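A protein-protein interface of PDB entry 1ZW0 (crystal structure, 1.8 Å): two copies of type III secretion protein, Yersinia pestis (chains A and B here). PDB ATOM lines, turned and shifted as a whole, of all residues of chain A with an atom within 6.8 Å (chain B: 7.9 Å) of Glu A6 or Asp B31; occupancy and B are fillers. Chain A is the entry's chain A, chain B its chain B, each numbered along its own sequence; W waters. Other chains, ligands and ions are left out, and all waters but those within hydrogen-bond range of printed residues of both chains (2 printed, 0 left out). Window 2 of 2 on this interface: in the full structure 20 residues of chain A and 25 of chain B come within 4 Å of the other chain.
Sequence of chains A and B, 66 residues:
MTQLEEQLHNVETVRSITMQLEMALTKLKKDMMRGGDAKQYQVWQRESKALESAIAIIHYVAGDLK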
ATOM      1  N   MET A   1      -8.504  -1.781  -4.567  1.00  0.00           N
ATOM      2  CA  MET A   1      -7.446  -1.190  -3.675  1.00  0.00           C
ATOM      3  C   MET A   1      -7.882   0.067  -2.944  1.00  0.00           C
ATOM      4  O   MET A   1      -7.341   0.356  -1.867  1.00  0.00           O
ATOM      5  CB  MET A   1      -6.199  -0.890  -4.447  1.00  0.00           C
ATOM      6  CG  MET A   1      -5.051  -0.185  -3.704  1.00  0.00           C
ATOM      7  SD  MET A   1      -4.410  -1.277  -2.458  1.00  0.00           S
ATOM      8  CE  MET A   1      -2.784  -1.481  -3.217  1.00  0.00           C
ATOM      9  N   THR A   2      -8.822   0.832  -3.512  1.00  0.00           N
ATOM     10  CA  THR A   2      -9.261   2.107  -2.901  1.00  0.00           C
ATOM     11  C   THR A   2      -9.960   1.701  -1.603  1.00  0.00           C
ATOM     12  O   THR A   2      -9.696   2.264  -0.522  1.00  0.00           O
ATOM     13  CB  THR A   2     -10.167   2.865  -3.867  1.00  0.00           C
ATOM     14  OG1 THR A   2      -9.367   3.467  -4.882  1.00  0.00           O
ATOM     15  CG2 THR A   2     -10.967   3.990  -3.232  1.00  0.00           C
ATOM     16  N   GLN A   3     -10.829   0.703  -1.695  1.00  0.00           N
ATOM     17  CA  GLN A   3     -11.523   0.219  -0.544  1.00  0.00           C
ATOM     18  C   GLN A   3     -10.595  -0.329   0.528  1.00  0.00           C
ATOM     19  O   GLN A   3     -10.815  -0.075   1.721  1.00  0.00           O
ATOM     20  CB  GLN A   3     -12.504  -0.850  -0.946  1.00  0.00           C
ATOM     21  CG  GLN A   3     -13.654  -0.273  -1.818  1.00  0.00           C
ATOM     22  CD  GLN A   3     -13.486  -0.585  -3.292  1.00  0.00           C
ATOM     23  OE1 GLN A   3     -12.388  -0.455  -3.865  1.00  0.00           O
ATOM     24  NE2 GLN A   3     -14.595  -1.012  -3.928  1.00  0.00           N
ATOM     25  N   LEU A   4      -9.581  -1.093   0.152  1.00  0.00           N
ATOM     26  CA  LEU A   4      -8.640  -1.600   1.121  1.00  0.00           C
ATOM     27  C   LEU A   4      -7.871  -0.497   1.849  1.00  0.00           C
ATOM     28  O   LEU A   4      -7.772  -0.492   3.067  1.00  0.00           O
ATOM     29  CB  LEU A   4      -7.646  -2.567   0.424  1.00  0.00           C
ATOM     30  CG  LEU A   4      -6.584  -3.187   1.299  1.00  0.00           C
ATOM     31  CD1 LEU A   4      -7.152  -3.858   2.590  1.00  0.00           C
ATOM     32  CD2 LEU A   4      -5.775  -4.199   0.458  1.00  0.00           C
ATOM     33  N   GLU A   5      -7.337   0.471   1.130  1.00  0.00           N
ATOM     34  CA  GLU A   5      -6.584   1.565   1.750  1.00  0.00           C
ATOM     35  C   GLU A   5      -7.497   2.370   2.716  1.00  0.00           C
ATOM     36  O   GLU A   5      -7.071   2.791   3.810  1.00  0.00           O
ATOM     37  CB  GLU A   5      -6.019   2.496   0.666  1.00  0.00           C
ATOM     38  CG  GLU A   5      -4.893   1.812  -0.056  1.00  0.00           C
ATOM     39  CD  GLU A   5      -4.182   2.634  -1.047  1.00  0.00           C
ATOM     40  OE1 GLU A   5      -4.878   3.342  -1.833  1.00  0.00           O
ATOM     41  OE2 GLU A   5      -2.918   2.543  -0.999  1.00  0.00           O
ATOM     42  N   GLU A   6      -8.703   2.611   2.297  1.00  0.00           N
ATOM     43  CA  GLU A   6      -9.617   3.404   3.106  1.00  0.00           C
ATOM     44  C   GLU A   6      -9.901   2.654   4.419  1.00  0.00           C
ATOM     45  O   GLU A   6      -9.933   3.287   5.499  1.00  0.00           O
ATOM     46  CB  GLU A   6     -10.841   3.662   2.281  1.00  0.00           C
ATOM     47  CG  GLU A   6     -12.090   3.941   3.031  1.00  0.00           C
ATOM     48  CD  GLU A   6     -13.220   4.224   2.117  1.00  0.00           C
ATOM     49  OE1 GLU A   6     -13.857   3.242   1.691  1.00  0.00           O
ATOM     50  OE2 GLU A   6     -13.537   5.398   1.887  1.00  0.00           O
ATOM     51  N   GLN A   7     -10.133   1.331   4.337  1.00  0.00           N
ATOM     52  CA  GLN A   7     -10.372   0.514   5.518  1.00  0.00           C
ATOM     53  C   GLN A   7      -9.146   0.521   6.446  1.00  0.00           C
ATOM     54  O   GLN A   7      -9.271   0.692   7.670  1.00  0.00           O
ATOM     55  CB  GLN A   7     -10.762  -0.922   5.161  1.00  0.00           C
ATOM     56  CG  GLN A   7     -10.976  -1.833   6.414  1.00  0.00           C
ATOM     57  CD  GLN A   7     -11.947  -3.028   6.175  1.00  0.00           C
ATOM     58  OE1 GLN A   7     -12.779  -3.001   5.266  1.00  0.00           O
ATOM     59  NE2 GLN A   7     -11.782  -4.082   6.946  1.00  0.00           N
ATOM     60  N   LEU A   8      -7.938   0.367   5.904  1.00  0.00           N
ATOM     61  CA  LEU A   8      -6.753   0.385   6.712  1.00  0.00           C
ATOM     62  C   LEU A   8      -6.599   1.717   7.427  1.00  0.00           C
ATOM     63  O   LEU A   8      -6.259   1.743   8.632  1.00  0.00           O
ATOM     64  CB  LEU A   8      -5.482   0.052   5.854  1.00  0.00           C
ATOM     65  CG  LEU A   8      -4.144   0.101   6.575  1.00  0.00           C
ATOM     66  CD1 LEU A   8      -3.957  -0.888   7.712  1.00  0.00           C
ATOM     67  CD2 LEU A   8      -3.012  -0.088   5.495  1.00  0.00           C
ATOM     68  N   HIS A   9      -6.800   2.815   6.718  1.00  0.00           N
ATOM     69  CA  HIS A   9      -6.654   4.126   7.330  1.00  0.00           C
ATOM     70  C   HIS A   9      -7.735   4.363   8.409  1.00  0.00           C
ATOM     71  O   HIS A   9      -7.444   4.965   9.425  1.00  0.00           O
ATOM     72  CB  HIS A   9      -6.742   5.194   6.315  1.00  0.00           C
ATOM     73  CG  HIS A   9      -5.648   5.123   5.298  1.00  0.00           C
ATOM     74  ND1 HIS A   9      -5.784   5.671   4.039  1.00  0.00           N
ATOM     75  CD2 HIS A   9      -4.431   4.529   5.335  1.00  0.00           C
ATOM     76  CE1 HIS A   9      -4.690   5.415   3.341  1.00  0.00           C
ATOM     77  NE2 HIS A   9      -3.843   4.748   4.097  1.00  0.00           N
ATOM     78  N   ASN A  10      -8.954   3.918   8.135  1.00  0.00           N
ATOM     79  CA  ASN A  10     -10.025   3.958   9.202  1.00  0.00           C
ATOM     80  C   ASN A  10      -9.683   3.177  10.445  1.00  0.00           C
ATOM     81  O   ASN A  10      -9.936   3.625  11.614  1.00  0.00           O
ATOM     82  CB  ASN A  10     -11.347   3.502   8.669  1.00  0.00           C
ATOM     83  CG  ASN A  10     -11.953   4.453   7.677  1.00  0.00           C
ATOM     84  OD1 ASN A  10     -11.644   5.642   7.620  1.00  0.00           O
ATOM     85  ND2 ASN A  10     -12.863   3.931   6.880  1.00  0.00           N
ATOM     86  N   VAL A  11      -9.138   1.967  10.272  1.00  0.00           N
ATOM     87  CA  VAL A  11      -8.663   1.174  11.413  1.00  0.00           C
ATOM     88  C   VAL A  11      -7.512   1.841  12.118  1.00  0.00           C
ATOM     89  O   VAL A  11      -7.440   1.804  13.336  1.00  0.00           O
ATOM     90  CB  VAL A  11      -8.314  -0.289  10.981  1.00  0.00           C
ATOM     91  CG1 VAL A  11      -7.667  -1.108  12.039  1.00  0.00           C
ATOM     92  CG2 VAL A  11      -9.532  -1.023  10.442  1.00  0.00           C
ATOM     93  N   ALA B  24     -15.293   7.579  14.804  1.00  0.00           N
ATOM     94  CA  ALA B  24     -14.271   6.862  14.018  1.00  0.00           C
ATOM     95  C   ALA B  24     -14.805   5.509  13.647  1.00  0.00           C
ATOM     96  O   ALA B  24     -14.571   4.986  12.562  1.00  0.00           O
ATOM     97  CB  ALA B  24     -12.985   6.706  14.820  1.00  0.00           C
ATOM     98  N   LEU B  25     -15.471   4.864  14.613  1.00  0.00           N
ATOM     99  CA  LEU B  25     -16.066   3.534  14.348  1.00  0.00           C
ATOM    100  C   LEU B  25     -17.218   3.653  13.356  1.00  0.00           C
ATOM    101  O   LEU B  25     -17.469   2.743  12.528  1.00  0.00           O
ATOM    102  CB  LEU B  25     -16.591   2.977  15.655  1.00  0.00           C
ATOM    103  CG  LEU B  25     -15.506   2.600  16.682  1.00  0.00           C
ATOM    104  CD1 LEU B  25     -16.187   2.365  18.059  1.00  0.00           C
ATOM    105  CD2 LEU B  25     -14.650   1.389  16.314  1.00  0.00           C
ATOM    106  N   THR B  26     -17.940   4.746  13.444  1.00  0.00           N
ATOM    107  CA  THR B  26     -19.073   5.014  12.511  1.00  0.00           C
ATOM    108  C   THR B  26     -18.514   5.122  11.069  1.00  0.00           C
ATOM    109  O   THR B  26     -19.105   4.591  10.122  1.00  0.00           O
ATOM    110  CB  THR B  26     -19.862   6.260  12.873  1.00  0.00           C
ATOM    111  OG1 THR B  26     -20.508   6.030  14.138  1.00  0.00           O
ATOM    112  CG2 THR B  26     -20.911   6.586  11.828  1.00  0.00           C
ATOM    113  N   LYS B  27     -17.448   5.881  10.919  1.00  0.00           N
ATOM    114  CA  LYS B  27     -16.811   6.032   9.563  1.00  0.00           C
ATOM    115  C   LYS B  27     -16.287   4.676   9.098  1.00  0.00           C
ATOM    116  O   LYS B  27     -16.514   4.262   7.969  1.00  0.00           O
ATOM    117  CB  LYS B  27     -15.669   7.013   9.649  1.00  0.00           C
ATOM    118  CG  LYS B  27     -14.800   7.123   8.350  1.00  0.00           C
ATOM    119  CD  LYS B  27     -14.222   8.529   8.224  1.00  0.00           C
ATOM    120  CE  LYS B  27     -13.645   8.813   6.842  1.00  0.00           C
ATOM    121  NZ  LYS B  27     -12.763   7.751   6.275  1.00  0.00           N
ATOM    122  N   LEU B  28     -15.627   3.946   9.955  1.00  0.00           N
ATOM    123  CA  LEU B  28     -15.190   2.608   9.633  1.00  0.00           C
ATOM    124  C   LEU B  28     -16.290   1.726   9.124  1.00  0.00           C
ATOM    125  O   LEU B  28     -16.129   1.082   8.062  1.00  0.00           O
ATOM    126  CB  LEU B  28     -14.544   1.931  10.827  1.00  0.00           C
ATOM    127  CG  LEU B  28     -14.066   0.499  10.713  1.00  0.00           C
ATOM    128  CD1 LEU B  28     -12.918   0.354   9.747  1.00  0.00           C
ATOM    129  CD2 LEU B  28     -13.581  -0.043  12.072  1.00  0.00           C
ATOM    130  N   LYS B  29     -17.385   1.652   9.866  1.00  0.00           N
ATOM    131  CA  LYS B  29     -18.519   0.818   9.490  1.00  0.00           C
ATOM    132  C   LYS B  29     -19.253   1.348   8.250  1.00  0.00           C
ATOM    133  O   LYS B  29     -19.655   0.577   7.373  1.00  0.00           O
ATOM    134  CB  LYS B  29     -19.457   0.623  10.713  1.00  0.00           C
ATOM    135  CG  LYS B  29     -20.377   1.723  11.078  1.00  0.00           C
ATOM    136  CD  LYS B  29     -21.779   1.178  11.479  1.00  0.00           C
ATOM    137  CE  LYS B  29     -22.749   2.301  11.683  1.00  0.00           C
ATOM    138  NZ  LYS B  29     -23.868   2.336  10.710  1.00  0.00           N
ATOM    139  N   LYS B  30     -19.462   2.644   8.156  1.00  0.00           N
ATOM    140  CA  LYS B  30     -20.116   3.211   6.967  1.00  0.00           C
ATOM    141  C   LYS B  30     -19.296   2.963   5.674  1.00  0.00           C
ATOM    142  O   LYS B  30     -19.881   2.627   4.612  1.00  0.00           O
ATOM    143  CB  LYS B  30     -20.303   4.691   7.110  1.00  0.00           C
ATOM    144  CG  LYS B  30     -20.581   5.373   5.796  1.00  0.00           C
ATOM    145  CD  LYS B  30     -21.002   6.827   5.935  1.00  0.00           C
ATOM    146  CE  LYS B  30     -21.246   7.448   4.550  1.00  0.00           C
ATOM    147  NZ  LYS B  30     -20.006   7.355   3.713  1.00  0.00           N
ATOM    148  N   ASP B  31     -17.984   3.204   5.759  1.00  0.00           N
ATOM    149  CA  ASP B  31     -17.086   3.068   4.608  1.00  0.00           C
ATOM    150  C   ASP B  31     -17.055   1.641   4.127  1.00  0.00           C
ATOM    151  O   ASP B  31     -17.037   1.388   2.903  1.00  0.00           O
ATOM    152  CB  ASP B  31     -15.683   3.643   4.873  1.00  0.00           C
ATOM    153  CG  ASP B  31     -15.668   5.196   4.871  1.00  0.00           C
ATOM    154  OD1 ASP B  31     -16.749   5.764   4.644  1.00  0.00           O
ATOM    155  OD2 ASP B  31     -14.606   5.820   5.145  1.00  0.00           O
ATOM    156  N   MET B  32     -17.081   0.683   5.051  1.00  0.00           N
ATOM    157  CA  MET B  32     -17.023  -0.705   4.611  1.00  0.00           C
ATOM    158  C   MET B  32     -18.360  -1.140   3.971  1.00  0.00           C
ATOM    159  O   MET B  32     -18.365  -2.001   3.083  1.00  0.00           O
ATOM    160  CB  MET B  32     -16.465  -1.631   5.711  1.00  0.00           C
ATOM    161  CG  MET B  32     -17.442  -2.320   6.511  1.00  0.00           C
ATOM    162  SD  MET B  32     -16.869  -3.099   8.054  1.00  0.00           S
ATOM    163  CE  MET B  32     -15.670  -1.975   8.657  1.00  0.00           C
ATOM    164  N   MET B  33     -19.483  -0.527   4.347  1.00  0.00           N
ATOM    165  CA  MET B  33     -20.717  -0.782   3.655  1.00  0.00           C
ATOM    166  C   MET B  33     -20.826   0.249   2.527  1.00  0.00           C
ATOM    167  O   MET B  33     -21.933   0.511   2.028  1.00  0.00           O
ATOM    168  CB  MET B  33     -21.917  -0.687   4.621  1.00  0.00           C
ATOM    169  CG  MET B  33     -21.873  -1.689   5.805  1.00  0.00           C
ATOM    170  SD  MET B  33     -21.702  -3.494   5.428  1.00  0.00           S
ATOM    171  CE  MET B  33     -20.058  -3.694   5.952  1.00  0.00           C
ATOM    172  N   SER B  48     -20.087  -4.943  10.571  1.00  0.00           N
ATOM    173  CA  SER B  48     -20.778  -3.669  10.650  1.00  0.00           C
ATOM    174  C   SER B  48     -21.805  -3.604  11.785  1.00  0.00           C
ATOM    175  O   SER B  48     -21.860  -2.605  12.512  1.00  0.00           O
ATOM    176  CB  SER B  48     -21.405  -3.322   9.293  1.00  0.00           C
ATOM    177  OG  SER B  48     -22.297  -2.254   9.455  1.00  0.00           O
HETATM  178  O   HOH W   1     -13.770   1.261   6.387  1.00  0.00           O
HETATM  179  O   HOH W   2     -12.131   5.807  11.363  1.00  0.00           O
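NZ of Lys B27 lies within salt-bridge range of OD2 of Asp B31 (2.9 Å). ND2 of Asn A10 sits close to O of Glu A6, 3.3 Å away. The side-chain amino group (NZ) of Lys B30 lies within salt-bridge range of the side-chain carboxylate (OD1) of Asp B31 (3.7 Å).
Glu A6 touches just one residue of chain B: Asp B31 (3.5 Å). Printed residues of chain B within 4 Å of Asn A10: Lys B27 (2.7 Å), Leu B28 (3.7 Å) and Asp B31 (3.1 Å). Of the printed residues of chain B, Val A11 touches Leu B28. Of the printed residues of chain A, Leu B28 touches Asn A10 (3.7 Å) and Val A11 (3.7 Å). Printed residues of chain A within 4 Å of Asp B31: Glu A6 (3.5 Å) and Asn A10 (3.1 Å).
Water W2 bridges the backbone carbonyl oxygen (O) of Ala B24 (2.8 Å) and the backbone carbonyl oxygen (O) of Asn A10 (3.1 Å). Water W1 lies within hydrogen-bond range of the side-chain amide nitrogen (ND2) of Asn A10 (2.9 Å) and the backbone carbonyl oxygen (O) of Leu B28 (2.9 Å).
OD1 of Asn A10 lies within hydrogen-bond range of NZ of Lys B27, 2.7 Å away. OD2 of Asp B31 lies close to OE2 of Glu A6 (3.5 Å). OD2 of Asp B31 sits at hydrogen-bond distance from ND2 of Asn A10 (3.1 Å).
Among the printed residues, 6 pairs touch across the chains. Among the printed residues, no Asp or Glu carboxylate lies within 4 Å of a Lys or Arg side-chain nitrogen of the other chain.
No position is printed for both chains. Of the 6 pairs that touch across the chains among the printed residues, none has its exchanged pair printed and touching as well.
Among the printed residues, pairs that only touch across the chains: Gln A7 with Met B32 (3.96 Å), Asn A10 with Leu B28 (3.7 Å) and Val A11 with Leu B28 (3.7 Å).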
